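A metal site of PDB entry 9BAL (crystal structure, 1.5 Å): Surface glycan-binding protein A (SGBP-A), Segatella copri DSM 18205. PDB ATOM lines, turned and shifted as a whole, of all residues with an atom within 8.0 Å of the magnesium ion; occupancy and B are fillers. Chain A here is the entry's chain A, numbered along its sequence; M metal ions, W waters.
NH1 of Arg 478 sits at hydrogen-bond distance from O of Thr 510, 2.8 Å away. ND2 of Asn 551 is in hydrogen-bond range of O of Asp 481, 2.9 Å away. O of Trp 474 sits at hydrogen-bond distance from NE of Arg 478 (3.0 Å).
The nearest printed residue that does not touch the magnesium ion is Asp 549 (4.2 Å).
OD1 of Asp 546 binds the magnesium ion (2.1 Å). OD1 of Asp 481 binds the magnesium ion (2.1 Å). The backbone carbonyl oxygen (O) of Ser 548 binds the magnesium ion. The magnesium ion is bound by O of Arg 478 (2.1 Å). Water W1 is bound to the magnesium ion (2.2 Å). The magnesium ion is bound by water W2. The magnesium ion has six donor atoms within binding distance.
Water W1 lies within hydrogen-bond range of OD2 of Asp 481 (2.7 Å), N of Ser 548 (3.0 Å), O of Arg 479 (3.2 Å) and N of Lys 547 (3.4 Å).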
ATOM      1  N   ASP A 200     -11.307  -5.284 -21.464  1.00  0.00           N
ATOM      2  CA  ASP A 200     -11.119  -6.588 -20.833  1.00  0.00           C
ATOM      3  C   ASP A 200      -9.684  -7.094 -20.960  1.00  0.00           C
ATOM      4  O   ASP A 200      -9.160  -7.700 -20.012  1.00  0.00           O
ATOM      5  CB  ASP A 200     -12.056  -7.634 -21.434  1.00  0.00           C
ATOM      6  CG  ASP A 200     -13.513  -7.367 -21.137  1.00  0.00           C
ATOM      7  OD1 ASP A 200     -13.813  -6.912 -20.019  1.00  0.00           O
ATOM      8  OD2 ASP A 200     -14.350  -7.633 -22.015  1.00  0.00           O
ATOM      9  N   TRP A 474     -21.714  -6.069 -33.871  1.00  0.00           N
ATOM     10  CA  TRP A 474     -21.015  -7.336 -33.721  1.00  0.00           C
ATOM     11  C   TRP A 474     -19.781  -7.182 -32.850  1.00  0.00           C
ATOM     12  O   TRP A 474     -19.512  -8.041 -31.996  1.00  0.00           O
ATOM     13  CB  TRP A 474     -20.657  -7.877 -35.104  1.00  0.00           C
ATOM     14  CG  TRP A 474     -20.136  -9.261 -35.150  1.00  0.00           C
ATOM     15  CD1 TRP A 474     -20.494 -10.329 -34.370  1.00  0.00           C
ATOM     16  CD2 TRP A 474     -19.170  -9.757 -36.085  1.00  0.00           C
ATOM     17  NE1 TRP A 474     -19.788 -11.454 -34.749  1.00  0.00           N
ATOM     18  CE2 TRP A 474     -18.977 -11.128 -35.822  1.00  0.00           C
ATOM     19  CE3 TRP A 474     -18.444  -9.154 -37.122  1.00  0.00           C
ATOM     20  CZ2 TRP A 474     -18.092 -11.914 -36.558  1.00  0.00           C
ATOM     21  CZ3 TRP A 474     -17.580  -9.952 -37.864  1.00  0.00           C
ATOM     22  CH2 TRP A 474     -17.401 -11.294 -37.572  1.00  0.00           C
ATOM     23  N   ALA A 475     -19.028  -6.089 -33.030  1.00  0.00           N
ATOM     24  CA  ALA A 475     -17.842  -5.896 -32.205  1.00  0.00           C
ATOM     25  C   ALA A 475     -18.215  -5.716 -30.726  1.00  0.00           C
ATOM     26  O   ALA A 475     -17.614  -6.329 -29.841  1.00  0.00           O
ATOM     27  CB  ALA A 475     -17.038  -4.701 -32.711  1.00  0.00           C
ATOM     28  N   ASN A 476     -19.193  -4.850 -30.439  1.00  0.00           N
ATOM     29  CA  ASN A 476     -19.523  -4.619 -29.036  1.00  0.00           C
ATOM     30  C   ASN A 476     -20.171  -5.844 -28.399  1.00  0.00           C
ATOM     31  O   ASN A 476     -19.985  -6.083 -27.201  1.00  0.00           O
ATOM     32  CB  ASN A 476     -20.453  -3.410 -28.883  1.00  0.00           C
ATOM     33  CG  ASN A 476     -20.604  -3.033 -27.434  1.00  0.00           C
ATOM     34  OD1 ASN A 476     -19.641  -2.598 -26.811  1.00  0.00           O
ATOM     35  ND2 ASN A 476     -21.787  -3.270 -26.867  1.00  0.00           N
ATOM     36  N   MET A 477     -20.930  -6.639 -29.170  1.00  0.00           N
ATOM     37  CA  MET A 477     -21.481  -7.858 -28.605  1.00  0.00           C
ATOM     38  C   MET A 477     -20.373  -8.852 -28.289  1.00  0.00           C
ATOM     39  O   MET A 477     -20.397  -9.500 -27.241  1.00  0.00           O
ATOM     40  CB  MET A 477     -22.501  -8.469 -29.559  1.00  0.00           C
ATOM     41  CG  MET A 477     -23.332  -9.539 -28.905  1.00  0.00           C
ATOM     42  SD  MET A 477     -24.552 -10.209 -30.048  1.00  0.00           S
ATOM     43  CE  MET A 477     -23.470 -10.806 -31.351  1.00  0.00           C
ATOM     44  N   ARG A 478     -19.368  -8.982 -29.172  1.00  0.00           N
ATOM     45  CA  ARG A 478     -18.259  -9.884 -28.880  1.00  0.00           C
ATOM     46  C   ARG A 478     -17.471  -9.401 -27.677  1.00  0.00           C
ATOM     47  O   ARG A 478     -17.014 -10.214 -26.861  1.00  0.00           O
ATOM     48  CB  ARG A 478     -17.350 -10.001 -30.104  1.00  0.00           C
ATOM     49  CG  ARG A 478     -17.934 -10.957 -31.154  1.00  0.00           C
ATOM     50  CD  ARG A 478     -17.112 -10.949 -32.431  1.00  0.00           C
ATOM     51  NE  ARG A 478     -17.206  -9.663 -33.111  1.00  0.00           N
ATOM     52  CZ  ARG A 478     -16.325  -9.217 -34.008  1.00  0.00           C
ATOM     53  NH1 ARG A 478     -15.288  -9.940 -34.374  1.00  0.00           N
ATOM     54  NH2 ARG A 478     -16.495  -8.001 -34.524  1.00  0.00           N
ATOM     55  N   ARG A 479     -17.293  -8.091 -27.549  1.00  0.00           N
ATOM     56  CA  ARG A 479     -16.505  -7.564 -26.432  1.00  0.00           C
ATOM     57  C   ARG A 479     -17.252  -7.715 -25.107  1.00  0.00           C
ATOM     58  O   ARG A 479     -16.686  -8.228 -24.137  1.00  0.00           O
ATOM     59  CB  ARG A 479     -16.166  -6.096 -26.697  1.00  0.00           C
ATOM     60  CG  ARG A 479     -15.144  -5.502 -25.728  1.00  0.00           C
ATOM     61  CD  ARG A 479     -15.738  -4.959 -24.426  1.00  0.00           C
ATOM     62  NE  ARG A 479     -16.826  -4.015 -24.651  1.00  0.00           N
ATOM     63  CZ  ARG A 479     -17.651  -3.598 -23.697  1.00  0.00           C
ATOM     64  NH1 ARG A 479     -17.488  -3.962 -22.429  1.00  0.00           N
ATOM     65  NH2 ARG A 479     -18.656  -2.789 -24.023  1.00  0.00           N
ATOM     66  N   SER A 480     -18.509  -7.262 -25.057  1.00  0.00           N
ATOM     67  CA  SER A 480     -19.242  -7.229 -23.801  1.00  0.00           C
ATOM     68  C   SER A 480     -19.903  -8.554 -23.459  1.00  0.00           C
ATOM     69  O   SER A 480     -20.295  -8.741 -22.302  1.00  0.00           O
ATOM     70  CB  SER A 480     -20.339  -6.154 -23.865  1.00  0.00           C
ATOM     71  OG  SER A 480     -21.375  -6.567 -24.746  1.00  0.00           O
ATOM     72  N   ASP A 481     -20.066  -9.419 -24.459  1.00  0.00           N
ATOM     73  CA  ASP A 481     -20.744 -10.710 -24.379  1.00  0.00           C
ATOM     74  C   ASP A 481     -22.228 -10.588 -24.082  1.00  0.00           C
ATOM     75  O   ASP A 481     -22.865 -11.565 -23.708  1.00  0.00           O
ATOM     76  CB  ASP A 481     -20.042 -11.626 -23.380  1.00  0.00           C
ATOM     77  CG  ASP A 481     -18.600 -11.820 -23.750  1.00  0.00           C
ATOM     78  OD1 ASP A 481     -18.335 -12.074 -24.948  1.00  0.00           O
ATOM     79  OD2 ASP A 481     -17.733 -11.634 -22.864  1.00  0.00           O
ATOM     80  N   TYR A 482     -22.811  -9.409 -24.323  1.00  0.00           N
ATOM     81  CA  TYR A 482     -24.241  -9.171 -24.261  1.00  0.00           C
ATOM     82  C   TYR A 482     -24.689  -8.480 -25.536  1.00  0.00           C
ATOM     83  O   TYR A 482     -23.881  -7.827 -26.205  1.00  0.00           O
ATOM     84  CB  TYR A 482     -24.582  -8.293 -23.045  1.00  0.00           C
ATOM     85  CG  TYR A 482     -24.369  -8.990 -21.737  1.00  0.00           C
ATOM     86  CD1 TYR A 482     -25.175 -10.055 -21.348  1.00  0.00           C
ATOM     87  CD2 TYR A 482     -23.354  -8.572 -20.877  1.00  0.00           C
ATOM     88  CE1 TYR A 482     -24.963 -10.692 -20.141  1.00  0.00           C
ATOM     89  CE2 TYR A 482     -23.150  -9.203 -19.670  1.00  0.00           C
ATOM     90  CZ  TYR A 482     -23.954 -10.263 -19.302  1.00  0.00           C
ATOM     91  OH  TYR A 482     -23.754 -10.900 -18.101  1.00  0.00           O
ATOM     92  N   MET A 508     -21.728 -18.778 -32.635  1.00  0.00           N
ATOM     93  CA  MET A 508     -21.673 -17.676 -33.570  1.00  0.00           C
ATOM     94  C   MET A 508     -20.206 -17.388 -33.848  1.00  0.00           C
ATOM     95  O   MET A 508     -19.399 -17.310 -32.898  1.00  0.00           O
ATOM     96  CB  MET A 508     -22.391 -16.443 -33.022  1.00  0.00           C
ATOM     97  CG  MET A 508     -21.987 -15.128 -33.678  1.00  0.00           C
ATOM     98  SD  MET A 508     -22.046 -13.614 -32.735  1.00  0.00           S
ATOM     99  CE  MET A 508     -20.557 -13.732 -31.762  1.00  0.00           C
ATOM    100  N   THR A 510     -16.672 -15.645 -34.348  1.00  0.00           N
ATOM    101  CA  THR A 510     -16.098 -14.496 -33.664  1.00  0.00           C
ATOM    102  C   THR A 510     -15.215 -13.646 -34.564  1.00  0.00           C
ATOM    103  O   THR A 510     -14.636 -12.665 -34.097  1.00  0.00           O
ATOM    104  CB  THR A 510     -15.317 -14.967 -32.456  1.00  0.00           C
ATOM    105  OG1 THR A 510     -14.500 -16.073 -32.838  1.00  0.00           O
ATOM    106  CG2 THR A 510     -16.280 -15.425 -31.354  1.00  0.00           C
ATOM    107  N   LYS A 542     -11.294 -16.297 -31.124  1.00  0.00           N
ATOM    108  CA  LYS A 542     -11.572 -14.952 -30.648  1.00  0.00           C
ATOM    109  C   LYS A 542     -10.391 -14.026 -30.928  1.00  0.00           C
ATOM    110  O   LYS A 542      -9.223 -14.437 -30.895  1.00  0.00           O
ATOM    111  CB  LYS A 542     -11.877 -14.973 -29.155  1.00  0.00           C
ATOM    112  CG  LYS A 542     -13.143 -15.766 -28.801  1.00  0.00           C
ATOM    113  CD  LYS A 542     -13.554 -15.586 -27.341  1.00  0.00           C
ATOM    114  CE  LYS A 542     -12.533 -16.200 -26.382  1.00  0.00           C
ATOM    115  NZ  LYS A 542     -12.194 -17.631 -26.654  1.00  0.00           N
ATOM    116  N   LEU A 543     -10.719 -12.759 -31.199  1.00  0.00           N
ATOM    117  CA  LEU A 543      -9.725 -11.722 -31.390  1.00  0.00           C
ATOM    118  C   LEU A 543      -9.116 -11.295 -30.058  1.00  0.00           C
ATOM    119  O   LEU A 543      -9.640 -11.577 -28.981  1.00  0.00           O
ATOM    120  CB  LEU A 543     -10.350 -10.545 -32.118  1.00  0.00           C
ATOM    121  CG  LEU A 543     -10.894 -10.909 -33.506  1.00  0.00           C
ATOM    122  CD1 LEU A 543     -11.422  -9.649 -34.180  1.00  0.00           C
ATOM    123  CD2 LEU A 543      -9.840 -11.582 -34.372  1.00  0.00           C
ATOM    124  N   TRP A 545      -8.946  -8.653 -28.248  1.00  0.00           N
ATOM    125  CA  TRP A 545      -9.723  -7.929 -27.242  1.00  0.00           C
ATOM    126  C   TRP A 545     -10.952  -8.695 -26.785  1.00  0.00           C
ATOM    127  O   TRP A 545     -11.666  -8.199 -25.920  1.00  0.00           O
ATOM    128  CB  TRP A 545     -10.162  -6.554 -27.762  1.00  0.00           C
ATOM    129  CG  TRP A 545     -10.702  -6.578 -29.174  1.00  0.00           C
ATOM    130  CD1 TRP A 545     -10.039  -6.233 -30.314  1.00  0.00           C
ATOM    131  CD2 TRP A 545     -12.022  -6.981 -29.593  1.00  0.00           C
ATOM    132  NE1 TRP A 545     -10.845  -6.384 -31.410  1.00  0.00           N
ATOM    133  CE2 TRP A 545     -12.071  -6.845 -31.004  1.00  0.00           C
ATOM    134  CE3 TRP A 545     -13.158  -7.440 -28.917  1.00  0.00           C
ATOM    135  CZ2 TRP A 545     -13.204  -7.145 -31.738  1.00  0.00           C
ATOM    136  CZ3 TRP A 545     -14.308  -7.729 -29.664  1.00  0.00           C
ATOM    137  CH2 TRP A 545     -14.307  -7.593 -31.066  1.00  0.00           C
ATOM    138  N   ASP A 546     -11.211  -9.873 -27.358  1.00  0.00           N
ATOM    139  CA  ASP A 546     -12.401 -10.655 -27.081  1.00  0.00           C
ATOM    140  C   ASP A 546     -11.992 -11.776 -26.132  1.00  0.00           C
ATOM    141  O   ASP A 546     -11.462 -12.800 -26.557  1.00  0.00           O
ATOM    142  CB  ASP A 546     -12.979 -11.179 -28.391  1.00  0.00           C
ATOM    143  CG  ASP A 546     -14.274 -11.912 -28.192  1.00  0.00           C
ATOM    144  OD1 ASP A 546     -14.727 -12.030 -27.040  1.00  0.00           O
ATOM    145  OD2 ASP A 546     -14.852 -12.377 -29.192  1.00  0.00           O
ATOM    146  N   LYS A 547     -12.249 -11.589 -24.847  1.00  0.00           N
ATOM    147  CA  LYS A 547     -11.739 -12.517 -23.840  1.00  0.00           C
ATOM    148  C   LYS A 547     -12.656 -13.713 -23.559  1.00  0.00           C
ATOM    149  O   LYS A 547     -12.148 -14.754 -23.117  1.00  0.00           O
ATOM    150  CB  LYS A 547     -11.477 -11.781 -22.518  1.00  0.00           C
ATOM    151  CG  LYS A 547     -10.331 -10.781 -22.613  1.00  0.00           C
ATOM    152  CD  LYS A 547      -9.103 -11.378 -23.288  1.00  0.00           C
ATOM    153  CE  LYS A 547      -8.447 -12.435 -22.417  1.00  0.00           C
ATOM    154  NZ  LYS A 547      -6.961 -12.432 -22.526  1.00  0.00           N
ATOM    155  N   SER A 548     -13.966 -13.591 -23.808  1.00  0.00           N
ATOM    156  CA  SER A 548     -14.919 -14.592 -23.345  1.00  0.00           C
ATOM    157  C   SER A 548     -15.975 -14.860 -24.419  1.00  0.00           C
ATOM    158  O   SER A 548     -16.151 -14.089 -25.348  1.00  0.00           O
ATOM    159  CB  SER A 548     -15.607 -14.148 -22.054  1.00  0.00           C
ATOM    160  OG  SER A 548     -14.658 -13.802 -21.052  1.00  0.00           O
ATOM    161  N   ASP A 549     -16.712 -15.947 -24.240  1.00  0.00           N
ATOM    162  CA  ASP A 549     -17.782 -16.298 -25.169  1.00  0.00           C
ATOM    163  C   ASP A 549     -19.014 -15.424 -24.940  1.00  0.00           C
ATOM    164  O   ASP A 549     -19.333 -15.050 -23.797  1.00  0.00           O
ATOM    165  CB  ASP A 549     -18.187 -17.764 -25.013  1.00  0.00           C
ATOM    166  CG  ASP A 549     -17.017 -18.712 -25.206  1.00  0.00           C
ATOM    167  OD1 ASP A 549     -16.007 -18.316 -25.828  1.00  0.00           O
ATOM    168  OD2 ASP A 549     -17.122 -19.880 -24.755  1.00  0.00           O
ATOM    169  N   VAL A 550     -19.727 -15.112 -26.021  1.00  0.00           N
ATOM    170  CA  VAL A 550     -20.986 -14.373 -25.879  1.00  0.00           C
ATOM    171  C   VAL A 550     -21.961 -15.209 -25.064  1.00  0.00           C
ATOM    172  O   VAL A 550     -22.012 -16.442 -25.183  1.00  0.00           O
ATOM    173  CB  VAL A 550     -21.555 -14.021 -27.263  1.00  0.00           C
ATOM    174  CG1 VAL A 550     -22.849 -13.226 -27.148  1.00  0.00           C
ATOM    175  CG2 VAL A 550     -20.546 -13.208 -28.066  1.00  0.00           C
ATOM    176  N   ASN A 551     -22.714 -14.540 -24.208  1.00  0.00           N
ATOM    177  CA  ASN A 551     -23.702 -15.237 -23.388  1.00  0.00           C
ATOM    178  C   ASN A 551     -24.847 -15.737 -24.250  1.00  0.00           C
ATOM    179  O   ASN A 551     -25.134 -15.184 -25.314  1.00  0.00           O
ATOM    180  CB  ASN A 551     -24.217 -14.300 -22.302  1.00  0.00           C
ATOM    181  CG  ASN A 551     -23.215 -14.113 -21.207  1.00  0.00           C
ATOM    182  OD1 ASN A 551     -22.961 -15.038 -20.436  1.00  0.00           O
ATOM    183  ND2 ASN A 551     -22.617 -12.933 -21.115  1.00  0.00           N
HETATM  184 MG    MG M   1     -16.605 -12.172 -26.138  1.00  0.00          MG
HETATM  185  O   HOH W   1     -15.601 -11.225 -24.475  1.00  0.00           O
HETATM  186  O   HOH W   2     -17.219 -13.012 -28.033  1.00  0.00           O
